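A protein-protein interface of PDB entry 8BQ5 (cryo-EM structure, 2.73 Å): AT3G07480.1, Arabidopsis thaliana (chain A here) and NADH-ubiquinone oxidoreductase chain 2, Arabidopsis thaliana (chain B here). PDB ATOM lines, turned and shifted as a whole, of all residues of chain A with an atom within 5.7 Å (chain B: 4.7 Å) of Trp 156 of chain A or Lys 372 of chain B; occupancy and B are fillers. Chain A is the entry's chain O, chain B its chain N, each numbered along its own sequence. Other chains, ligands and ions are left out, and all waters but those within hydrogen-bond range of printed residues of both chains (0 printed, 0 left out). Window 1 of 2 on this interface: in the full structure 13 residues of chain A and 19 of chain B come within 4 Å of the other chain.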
ATOM      1  N   ASP A  79      -3.592   3.125  -6.302  1.00  0.00           N
ATOM      2  CA  ASP A  79      -2.868   1.984  -6.840  1.00  0.00           C
ATOM      3  C   ASP A  79      -1.586   2.462  -7.512  1.00  0.00           C
ATOM      4  O   ASP A  79      -1.652   3.295  -8.429  1.00  0.00           O
ATOM      5  CB  ASP A  79      -3.742   1.233  -7.839  1.00  0.00           C
ATOM      6  CG  ASP A  79      -3.188  -0.133  -8.196  1.00  0.00           C
ATOM      7  OD1 ASP A  79      -2.111  -0.503  -7.687  1.00  0.00           O
ATOM      8  OD2 ASP A  79      -3.830  -0.837  -9.000  1.00  0.00           O
ATOM      9  N   ALA A  81       0.244   0.893  -9.614  1.00  0.00           N
ATOM     10  CA  ALA A  81       0.236   0.478 -11.012  1.00  0.00           C
ATOM     11  C   ALA A  81      -0.515   1.454 -11.906  1.00  0.00           C
ATOM     12  O   ALA A  81      -0.209   1.548 -13.100  1.00  0.00           O
ATOM     13  CB  ALA A  81      -0.377  -0.918 -11.140  1.00  0.00           C
ATOM     14  N   SER A  82      -1.488   2.183 -11.362  1.00  0.00           N
ATOM     15  CA  SER A  82      -2.274   3.113 -12.160  1.00  0.00           C
ATOM     16  C   SER A  82      -1.523   4.394 -12.494  1.00  0.00           C
ATOM     17  O   SER A  82      -1.949   5.130 -13.389  1.00  0.00           O
ATOM     18  CB  SER A  82      -3.567   3.463 -11.425  1.00  0.00           C
ATOM     19  OG  SER A  82      -3.336   4.477 -10.466  1.00  0.00           O
ATOM     20  N   ARG A  84       2.571   5.225 -12.592  1.00  0.00           N
ATOM     21  CA  ARG A  84       3.915   4.737 -12.306  1.00  0.00           C
ATOM     22  C   ARG A  84       4.986   5.813 -12.409  1.00  0.00           C
ATOM     23  O   ARG A  84       6.057   5.658 -11.813  1.00  0.00           O
ATOM     24  CB  ARG A  84       4.262   3.575 -13.242  1.00  0.00           C
ATOM     25  CG  ARG A  84       3.701   2.238 -12.780  1.00  0.00           C
ATOM     26  CD  ARG A  84       4.053   1.119 -13.744  1.00  0.00           C
ATOM     27  NE  ARG A  84       3.506   1.362 -15.073  1.00  0.00           N
ATOM     28  CZ  ARG A  84       3.655   0.548 -16.109  1.00  0.00           C
ATOM     29  NH1 ARG A  84       4.316  -0.591 -16.002  1.00  0.00           N
ATOM     30  NH2 ARG A  84       3.130   0.888 -17.281  1.00  0.00           N
ATOM     31  N   SER A  92      -3.502  10.839 -16.430  1.00  0.00           N
ATOM     32  CA  SER A  92      -4.897  10.995 -16.820  1.00  0.00           C
ATOM     33  C   SER A  92      -5.748  11.288 -15.593  1.00  0.00           C
ATOM     34  O   SER A  92      -6.883  10.826 -15.472  1.00  0.00           O
ATOM     35  CB  SER A  92      -5.413   9.759 -17.553  1.00  0.00           C
ATOM     36  OG  SER A  92      -4.816   9.626 -18.829  1.00  0.00           O
ATOM     37  N   GLU A  94      -5.345  10.078 -12.718  1.00  0.00           N
ATOM     38  CA  GLU A  94      -5.408   8.969 -11.773  1.00  0.00           C
ATOM     39  C   GLU A  94      -4.955   9.397 -10.387  1.00  0.00           C
ATOM     40  O   GLU A  94      -5.390   8.814  -9.389  1.00  0.00           O
ATOM     41  CB  GLU A  94      -4.545   7.805 -12.256  1.00  0.00           C
ATOM     42  CG  GLU A  94      -4.933   7.243 -13.609  1.00  0.00           C
ATOM     43  CD  GLU A  94      -4.163   7.880 -14.749  1.00  0.00           C
ATOM     44  OE1 GLU A  94      -3.501   8.917 -14.524  1.00  0.00           O
ATOM     45  OE2 GLU A  94      -4.208   7.333 -15.869  1.00  0.00           O
ATOM     46  N   LYS A 154     -10.767   6.329 -11.179  1.00  0.00           N
ATOM     47  CA  LYS A 154     -11.202   6.203 -12.557  1.00  0.00           C
ATOM     48  C   LYS A 154     -10.610   4.943 -13.188  1.00  0.00           C
ATOM     49  O   LYS A 154      -9.562   4.460 -12.754  1.00  0.00           O
ATOM     50  CB  LYS A 154     -10.779   7.425 -13.366  1.00  0.00           C
ATOM     51  CG  LYS A 154     -10.773   8.734 -12.595  1.00  0.00           C
ATOM     52  CD  LYS A 154     -10.021   9.808 -13.370  1.00  0.00           C
ATOM     53  CE  LYS A 154     -10.330  11.198 -12.845  1.00  0.00           C
ATOM     54  NZ  LYS A 154      -9.915  11.360 -11.429  1.00  0.00           N
ATOM     55  N   PRO A 155     -11.270   4.381 -14.201  1.00  0.00           N
ATOM     56  CA  PRO A 155     -10.643   3.296 -14.962  1.00  0.00           C
ATOM     57  C   PRO A 155      -9.385   3.792 -15.657  1.00  0.00           C
ATOM     58  O   PRO A 155      -9.343   4.907 -16.183  1.00  0.00           O
ATOM     59  CB  PRO A 155     -11.730   2.903 -15.968  1.00  0.00           C
ATOM     60  CG  PRO A 155     -12.527   4.163 -16.126  1.00  0.00           C
ATOM     61  CD  PRO A 155     -12.609   4.694 -14.725  1.00  0.00           C
ATOM     62  N   TRP A 156      -8.348   2.956 -15.656  1.00  0.00           N
ATOM     63  CA  TRP A 156      -7.074   3.355 -16.246  1.00  0.00           C
ATOM     64  C   TRP A 156      -6.413   2.294 -17.110  1.00  0.00           C
ATOM     65  O   TRP A 156      -5.514   2.642 -17.883  1.00  0.00           O
ATOM     66  CB  TRP A 156      -6.090   3.772 -15.145  1.00  0.00           C
ATOM     67  CG  TRP A 156      -5.865   2.698 -14.141  1.00  0.00           C
ATOM     68  CD1 TRP A 156      -6.553   2.509 -12.982  1.00  0.00           C
ATOM     69  CD2 TRP A 156      -4.900   1.645 -14.211  1.00  0.00           C
ATOM     70  NE1 TRP A 156      -6.072   1.409 -12.320  1.00  0.00           N
ATOM     71  CE2 TRP A 156      -5.056   0.859 -13.056  1.00  0.00           C
ATOM     72  CE3 TRP A 156      -3.914   1.293 -15.138  1.00  0.00           C
ATOM     73  CZ2 TRP A 156      -4.264  -0.254 -12.799  1.00  0.00           C
ATOM     74  CZ3 TRP A 156      -3.131   0.187 -14.883  1.00  0.00           C
ATOM     75  CH2 TRP A 156      -3.310  -0.575 -13.723  1.00  0.00           C
ATOM     76  N   ASP A 157      -6.817   1.030 -17.034  1.00  0.00           N
ATOM     77  CA  ASP A 157      -6.110  -0.060 -17.705  1.00  0.00           C
ATOM     78  C   ASP A 157      -6.697  -0.240 -19.100  1.00  0.00           C
ATOM     79  O   ASP A 157      -7.611  -1.034 -19.314  1.00  0.00           O
ATOM     80  CB  ASP A 157      -6.209  -1.335 -16.881  1.00  0.00           C
ATOM     81  CG  ASP A 157      -5.188  -2.374 -17.284  1.00  0.00           C
ATOM     82  OD1 ASP A 157      -4.262  -2.035 -18.047  1.00  0.00           O
ATOM     83  OD2 ASP A 157      -5.315  -3.532 -16.838  1.00  0.00           O
ATOM     84  N   ILE A 158      -6.160   0.502 -20.063  1.00  0.00           N
ATOM     85  CA  ILE A 158      -6.623   0.449 -21.448  1.00  0.00           C
ATOM     86  C   ILE A 158      -6.330  -0.943 -22.004  1.00  0.00           C
ATOM     87  O   ILE A 158      -5.184  -1.411 -21.922  1.00  0.00           O
ATOM     88  CB  ILE A 158      -5.933   1.527 -22.295  1.00  0.00           C
ATOM     89  CG1 ILE A 158      -6.502   2.916 -22.004  1.00  0.00           C
ATOM     90  CG2 ILE A 158      -6.052   1.185 -23.779  1.00  0.00           C
ATOM     91  CD1 ILE A 158      -7.531   3.314 -22.811  1.00  0.00           C
ATOM     92  N   PHE B 171     -13.521   0.419 -20.869  1.00  0.00           N
ATOM     93  CA  PHE B 171     -13.021   0.861 -22.163  1.00  0.00           C
ATOM     94  C   PHE B 171     -13.494  -0.056 -23.286  1.00  0.00           C
ATOM     95  O   PHE B 171     -13.942   0.413 -24.337  1.00  0.00           O
ATOM     96  CB  PHE B 171     -11.496   0.937 -22.123  1.00  0.00           C
ATOM     97  CG  PHE B 171     -10.965   1.870 -21.073  1.00  0.00           C
ATOM     98  CD1 PHE B 171     -11.128   3.238 -21.199  1.00  0.00           C
ATOM     99  CD2 PHE B 171     -10.306   1.380 -19.957  1.00  0.00           C
ATOM    100  CE1 PHE B 171     -10.639   4.102 -20.237  1.00  0.00           C
ATOM    101  CE2 PHE B 171      -9.816   2.239 -18.991  1.00  0.00           C
ATOM    102  CZ  PHE B 171      -9.984   3.602 -19.132  1.00  0.00           C
ATOM    103  N   LYS B 314      -0.711   9.376 -25.844  1.00  0.00           N
ATOM    104  CA  LYS B 314      -0.771   7.931 -25.697  1.00  0.00           C
ATOM    105  C   LYS B 314      -0.449   7.260 -27.024  1.00  0.00           C
ATOM    106  O   LYS B 314      -0.760   7.785 -28.097  1.00  0.00           O
ATOM    107  CB  LYS B 314      -2.145   7.474 -25.193  1.00  0.00           C
ATOM    108  CG  LYS B 314      -2.499   8.005 -23.816  1.00  0.00           C
ATOM    109  CD  LYS B 314      -3.796   7.401 -23.310  1.00  0.00           C
ATOM    110  CE  LYS B 314      -4.971   8.319 -23.581  1.00  0.00           C
ATOM    111  NZ  LYS B 314      -6.264   7.684 -23.214  1.00  0.00           N
ATOM    112  N   VAL B 315       0.177   6.088 -26.934  1.00  0.00           N
ATOM    113  CA  VAL B 315       0.758   5.453 -28.114  1.00  0.00           C
ATOM    114  C   VAL B 315      -0.332   4.996 -29.078  1.00  0.00           C
ATOM    115  O   VAL B 315      -0.250   5.234 -30.291  1.00  0.00           O
ATOM    116  CB  VAL B 315       1.668   4.287 -27.686  1.00  0.00           C
ATOM    117  CG1 VAL B 315       2.228   3.571 -28.901  1.00  0.00           C
ATOM    118  CG2 VAL B 315       2.780   4.786 -26.775  1.00  0.00           C
ATOM    119  N   ARG B 370       2.429  -3.210 -19.674  1.00  0.00           N
ATOM    120  CA  ARG B 370       1.321  -2.251 -19.651  1.00  0.00           C
ATOM    121  C   ARG B 370       1.757  -0.860 -20.113  1.00  0.00           C
ATOM    122  O   ARG B 370       1.526   0.141 -19.435  1.00  0.00           O
ATOM    123  CB  ARG B 370       0.684  -2.178 -18.261  1.00  0.00           C
ATOM    124  CG  ARG B 370      -0.079  -3.415 -17.870  1.00  0.00           C
ATOM    125  CD  ARG B 370      -1.415  -3.471 -18.570  1.00  0.00           C
ATOM    126  NE  ARG B 370      -2.172  -4.647 -18.165  1.00  0.00           N
ATOM    127  CZ  ARG B 370      -1.898  -5.884 -18.556  1.00  0.00           C
ATOM    128  NH1 ARG B 370      -0.912  -6.140 -19.402  1.00  0.00           N
ATOM    129  NH2 ARG B 370      -2.631  -6.889 -18.090  1.00  0.00           N
ATOM    130  N   VAL B 371       2.381  -0.799 -21.293  1.00  0.00           N
ATOM    131  CA  VAL B 371       2.725   0.498 -21.862  1.00  0.00           C
ATOM    132  C   VAL B 371       1.445   1.237 -22.226  1.00  0.00           C
ATOM    133  O   VAL B 371       0.539   0.683 -22.862  1.00  0.00           O
ATOM    134  CB  VAL B 371       3.670   0.336 -23.066  1.00  0.00           C
ATOM    135  CG1 VAL B 371       2.961  -0.297 -24.257  1.00  0.00           C
ATOM    136  CG2 VAL B 371       4.267   1.678 -23.455  1.00  0.00           C
ATOM    137  N   LYS B 372       1.341   2.467 -21.775  1.00  0.00           N
ATOM    138  CA  LYS B 372       0.156   3.267 -22.060  1.00  0.00           C
ATOM    139  C   LYS B 372       0.486   4.641 -22.620  1.00  0.00           C
ATOM    140  O   LYS B 372      -0.202   5.107 -23.530  1.00  0.00           O
ATOM    141  CB  LYS B 372      -0.682   3.407 -20.782  1.00  0.00           C
ATOM    142  CG  LYS B 372      -1.958   4.200 -20.952  1.00  0.00           C
ATOM    143  CD  LYS B 372      -2.664   4.373 -19.619  1.00  0.00           C
ATOM    144  CE  LYS B 372      -3.823   5.343 -19.739  1.00  0.00           C
ATOM    145  NZ  LYS B 372      -4.565   5.487 -18.462  1.00  0.00           N
ATOM    146  N   TYR B 373       1.528   5.290 -22.114  1.00  0.00           N
ATOM    147  CA  TYR B 373       1.888   6.639 -22.519  1.00  0.00           C
ATOM    148  C   TYR B 373       3.178   6.621 -23.325  1.00  0.00           C
ATOM    149  O   TYR B 373       3.980   5.688 -23.225  1.00  0.00           O
ATOM    150  CB  TYR B 373       2.063   7.556 -21.308  1.00  0.00           C
ATOM    151  CG  TYR B 373       0.833   7.700 -20.445  1.00  0.00           C
ATOM    152  CD1 TYR B 373      -0.189   8.565 -20.805  1.00  0.00           C
ATOM    153  CD2 TYR B 373       0.706   6.989 -19.260  1.00  0.00           C
ATOM    154  CE1 TYR B 373      -1.312   8.708 -20.017  1.00  0.00           C
ATOM    155  CE2 TYR B 373      -0.411   7.126 -18.466  1.00  0.00           C
ATOM    156  CZ  TYR B 373      -1.418   7.986 -18.849  1.00  0.00           C
ATOM    157  OH  TYR B 373      -2.532   8.124 -18.058  1.00  0.00           O
ATOM    158  N   ILE B 374       3.371   7.667 -24.129  1.00  0.00           N
ATOM    159  CA  ILE B 374       4.632   7.826 -24.847  1.00  0.00           C
ATOM    160  C   ILE B 374       5.778   7.998 -23.858  1.00  0.00           C
ATOM    161  O   ILE B 374       6.883   7.481 -24.065  1.00  0.00           O
ATOM    162  CB  ILE B 374       4.545   9.007 -25.830  1.00  0.00           C
ATOM    163  CG1 ILE B 374       3.628   8.660 -27.005  1.00  0.00           C
ATOM    164  CG2 ILE B 374       5.923   9.389 -26.341  1.00  0.00           C
ATOM    165  CD1 ILE B 374       2.915   9.859 -27.581  1.00  0.00           C
ATOM    166  N   ASP B 376       6.191   6.530 -21.201  1.00  0.00           N
ATOM    167  CA  ASP B 376       6.595   5.237 -20.661  1.00  0.00           C
ATOM    168  C   ASP B 376       7.788   4.653 -21.405  1.00  0.00           C
ATOM    169  O   ASP B 376       8.422   3.720 -20.903  1.00  0.00           O
ATOM    170  CB  ASP B 376       5.425   4.253 -20.713  1.00  0.00           C
ATOM    171  CG  ASP B 376       4.287   4.644 -19.791  1.00  0.00           C
ATOM    172  OD1 ASP B 376       4.518   5.430 -18.850  1.00  0.00           O
ATOM    173  OD2 ASP B 376       3.157   4.158 -20.008  1.00  0.00           O
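Phe 171 of chain B touches Pro 155 of chain A (CZ to O, 3.3 Å).
N of Trp 156 of chain A touches CE2 of Phe 171 of chain B (3.7 Å).
Asp 157 of chain A touches Phe 171 of chain B (O to CD2, 3.7 Å).
Ile 158 of chain A touches Phe 171 of chain B.
NZ of Lys 372 of chain B sits at hydrogen-bond distance from OH of Tyr 373 of chain B, 3.4 Å away.
The side-chain carboxylate (OD2) of Asp 376 of chain B sits at hydrogen-bond distance from the backbone NH (N) of Tyr 373 of chain B, 2.9 Å away.
N of Ser 92 of chain A is in hydrogen-bond range of OE1 of Glu 94 of chain A, 2.7 Å away.
OD2 of Asp 376 of chain B is in hydrogen-bond range of N of Lys 372 of chain B, 3.0 Å away.
The side-chain hydroxyl (OG) of Ser 92 of chain A lies within hydrogen-bond range of the side-chain hydroxyl (OH) of Tyr 373 of chain B (2.8 Å).
O of Arg 370 of chain B sits at hydrogen-bond distance from NH2 of Arg 84 of chain A, 2.8 Å away.
The guanidinium group of Arg 370 of chain B lies within salt-bridge range of the side-chain carboxylate of Asp 157 of chain A (3.3 Å).
The side-chain amino group (NZ) of Lys 372 of chain B lies within salt-bridge range of the side-chain carboxylate (OE2) of Glu 94 of chain A (3.2 Å).
The backbone carbonyl oxygen of Trp 156 of chain A is in hydrogen-bond range of the side-chain amino group of Lys 372 of chain B (3.1 Å).
OH of Tyr 373 of chain B lies within hydrogen-bond range of OE2 of Glu 94 of chain A (2.9 Å).
Along chain B the printed residues that touch a printed residue of chain A span positions 171 to 373.
Of chain B, only Phe 171 (3.7 Å) and Lys 372 (3.1 Å) come within 4 Å of Trp 156 of chain A.
Lys 372 of chain B touches just these residues of chain A: Glu 94 (3.2 Å) and Trp 156 (3.1 Å).
Of the printed residues of chain B, Glu 94 of chain A touches Lys 372 and Tyr 373.
Of the printed residues of chain B, Ser 92 of chain A touches Tyr 373 (2.8 Å).
Printed residues of chain B within 4 Å of Asp 157 of chain A: Phe 171 and Arg 370.
Of the printed residues of chain B, Ile 158 of chain A touches Phe 171.
Of the printed residues of chain A, Arg 370 of chain B touches Arg 84 (2.8 Å) and Asp 157 (3.2 Å).
Ala 81 of chain A touches none of the printed residues of chain B.
Val 371 of chain B touches none of the printed residues of chain A.
The nearest residue of chain A that does not touch Lys 372 of chain B is Ser 92 of chain A (4.2 Å).
The nearest printed residue of chain B that does not touch Asp 157 of chain A is Lys 372 of chain B (5.2 Å).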
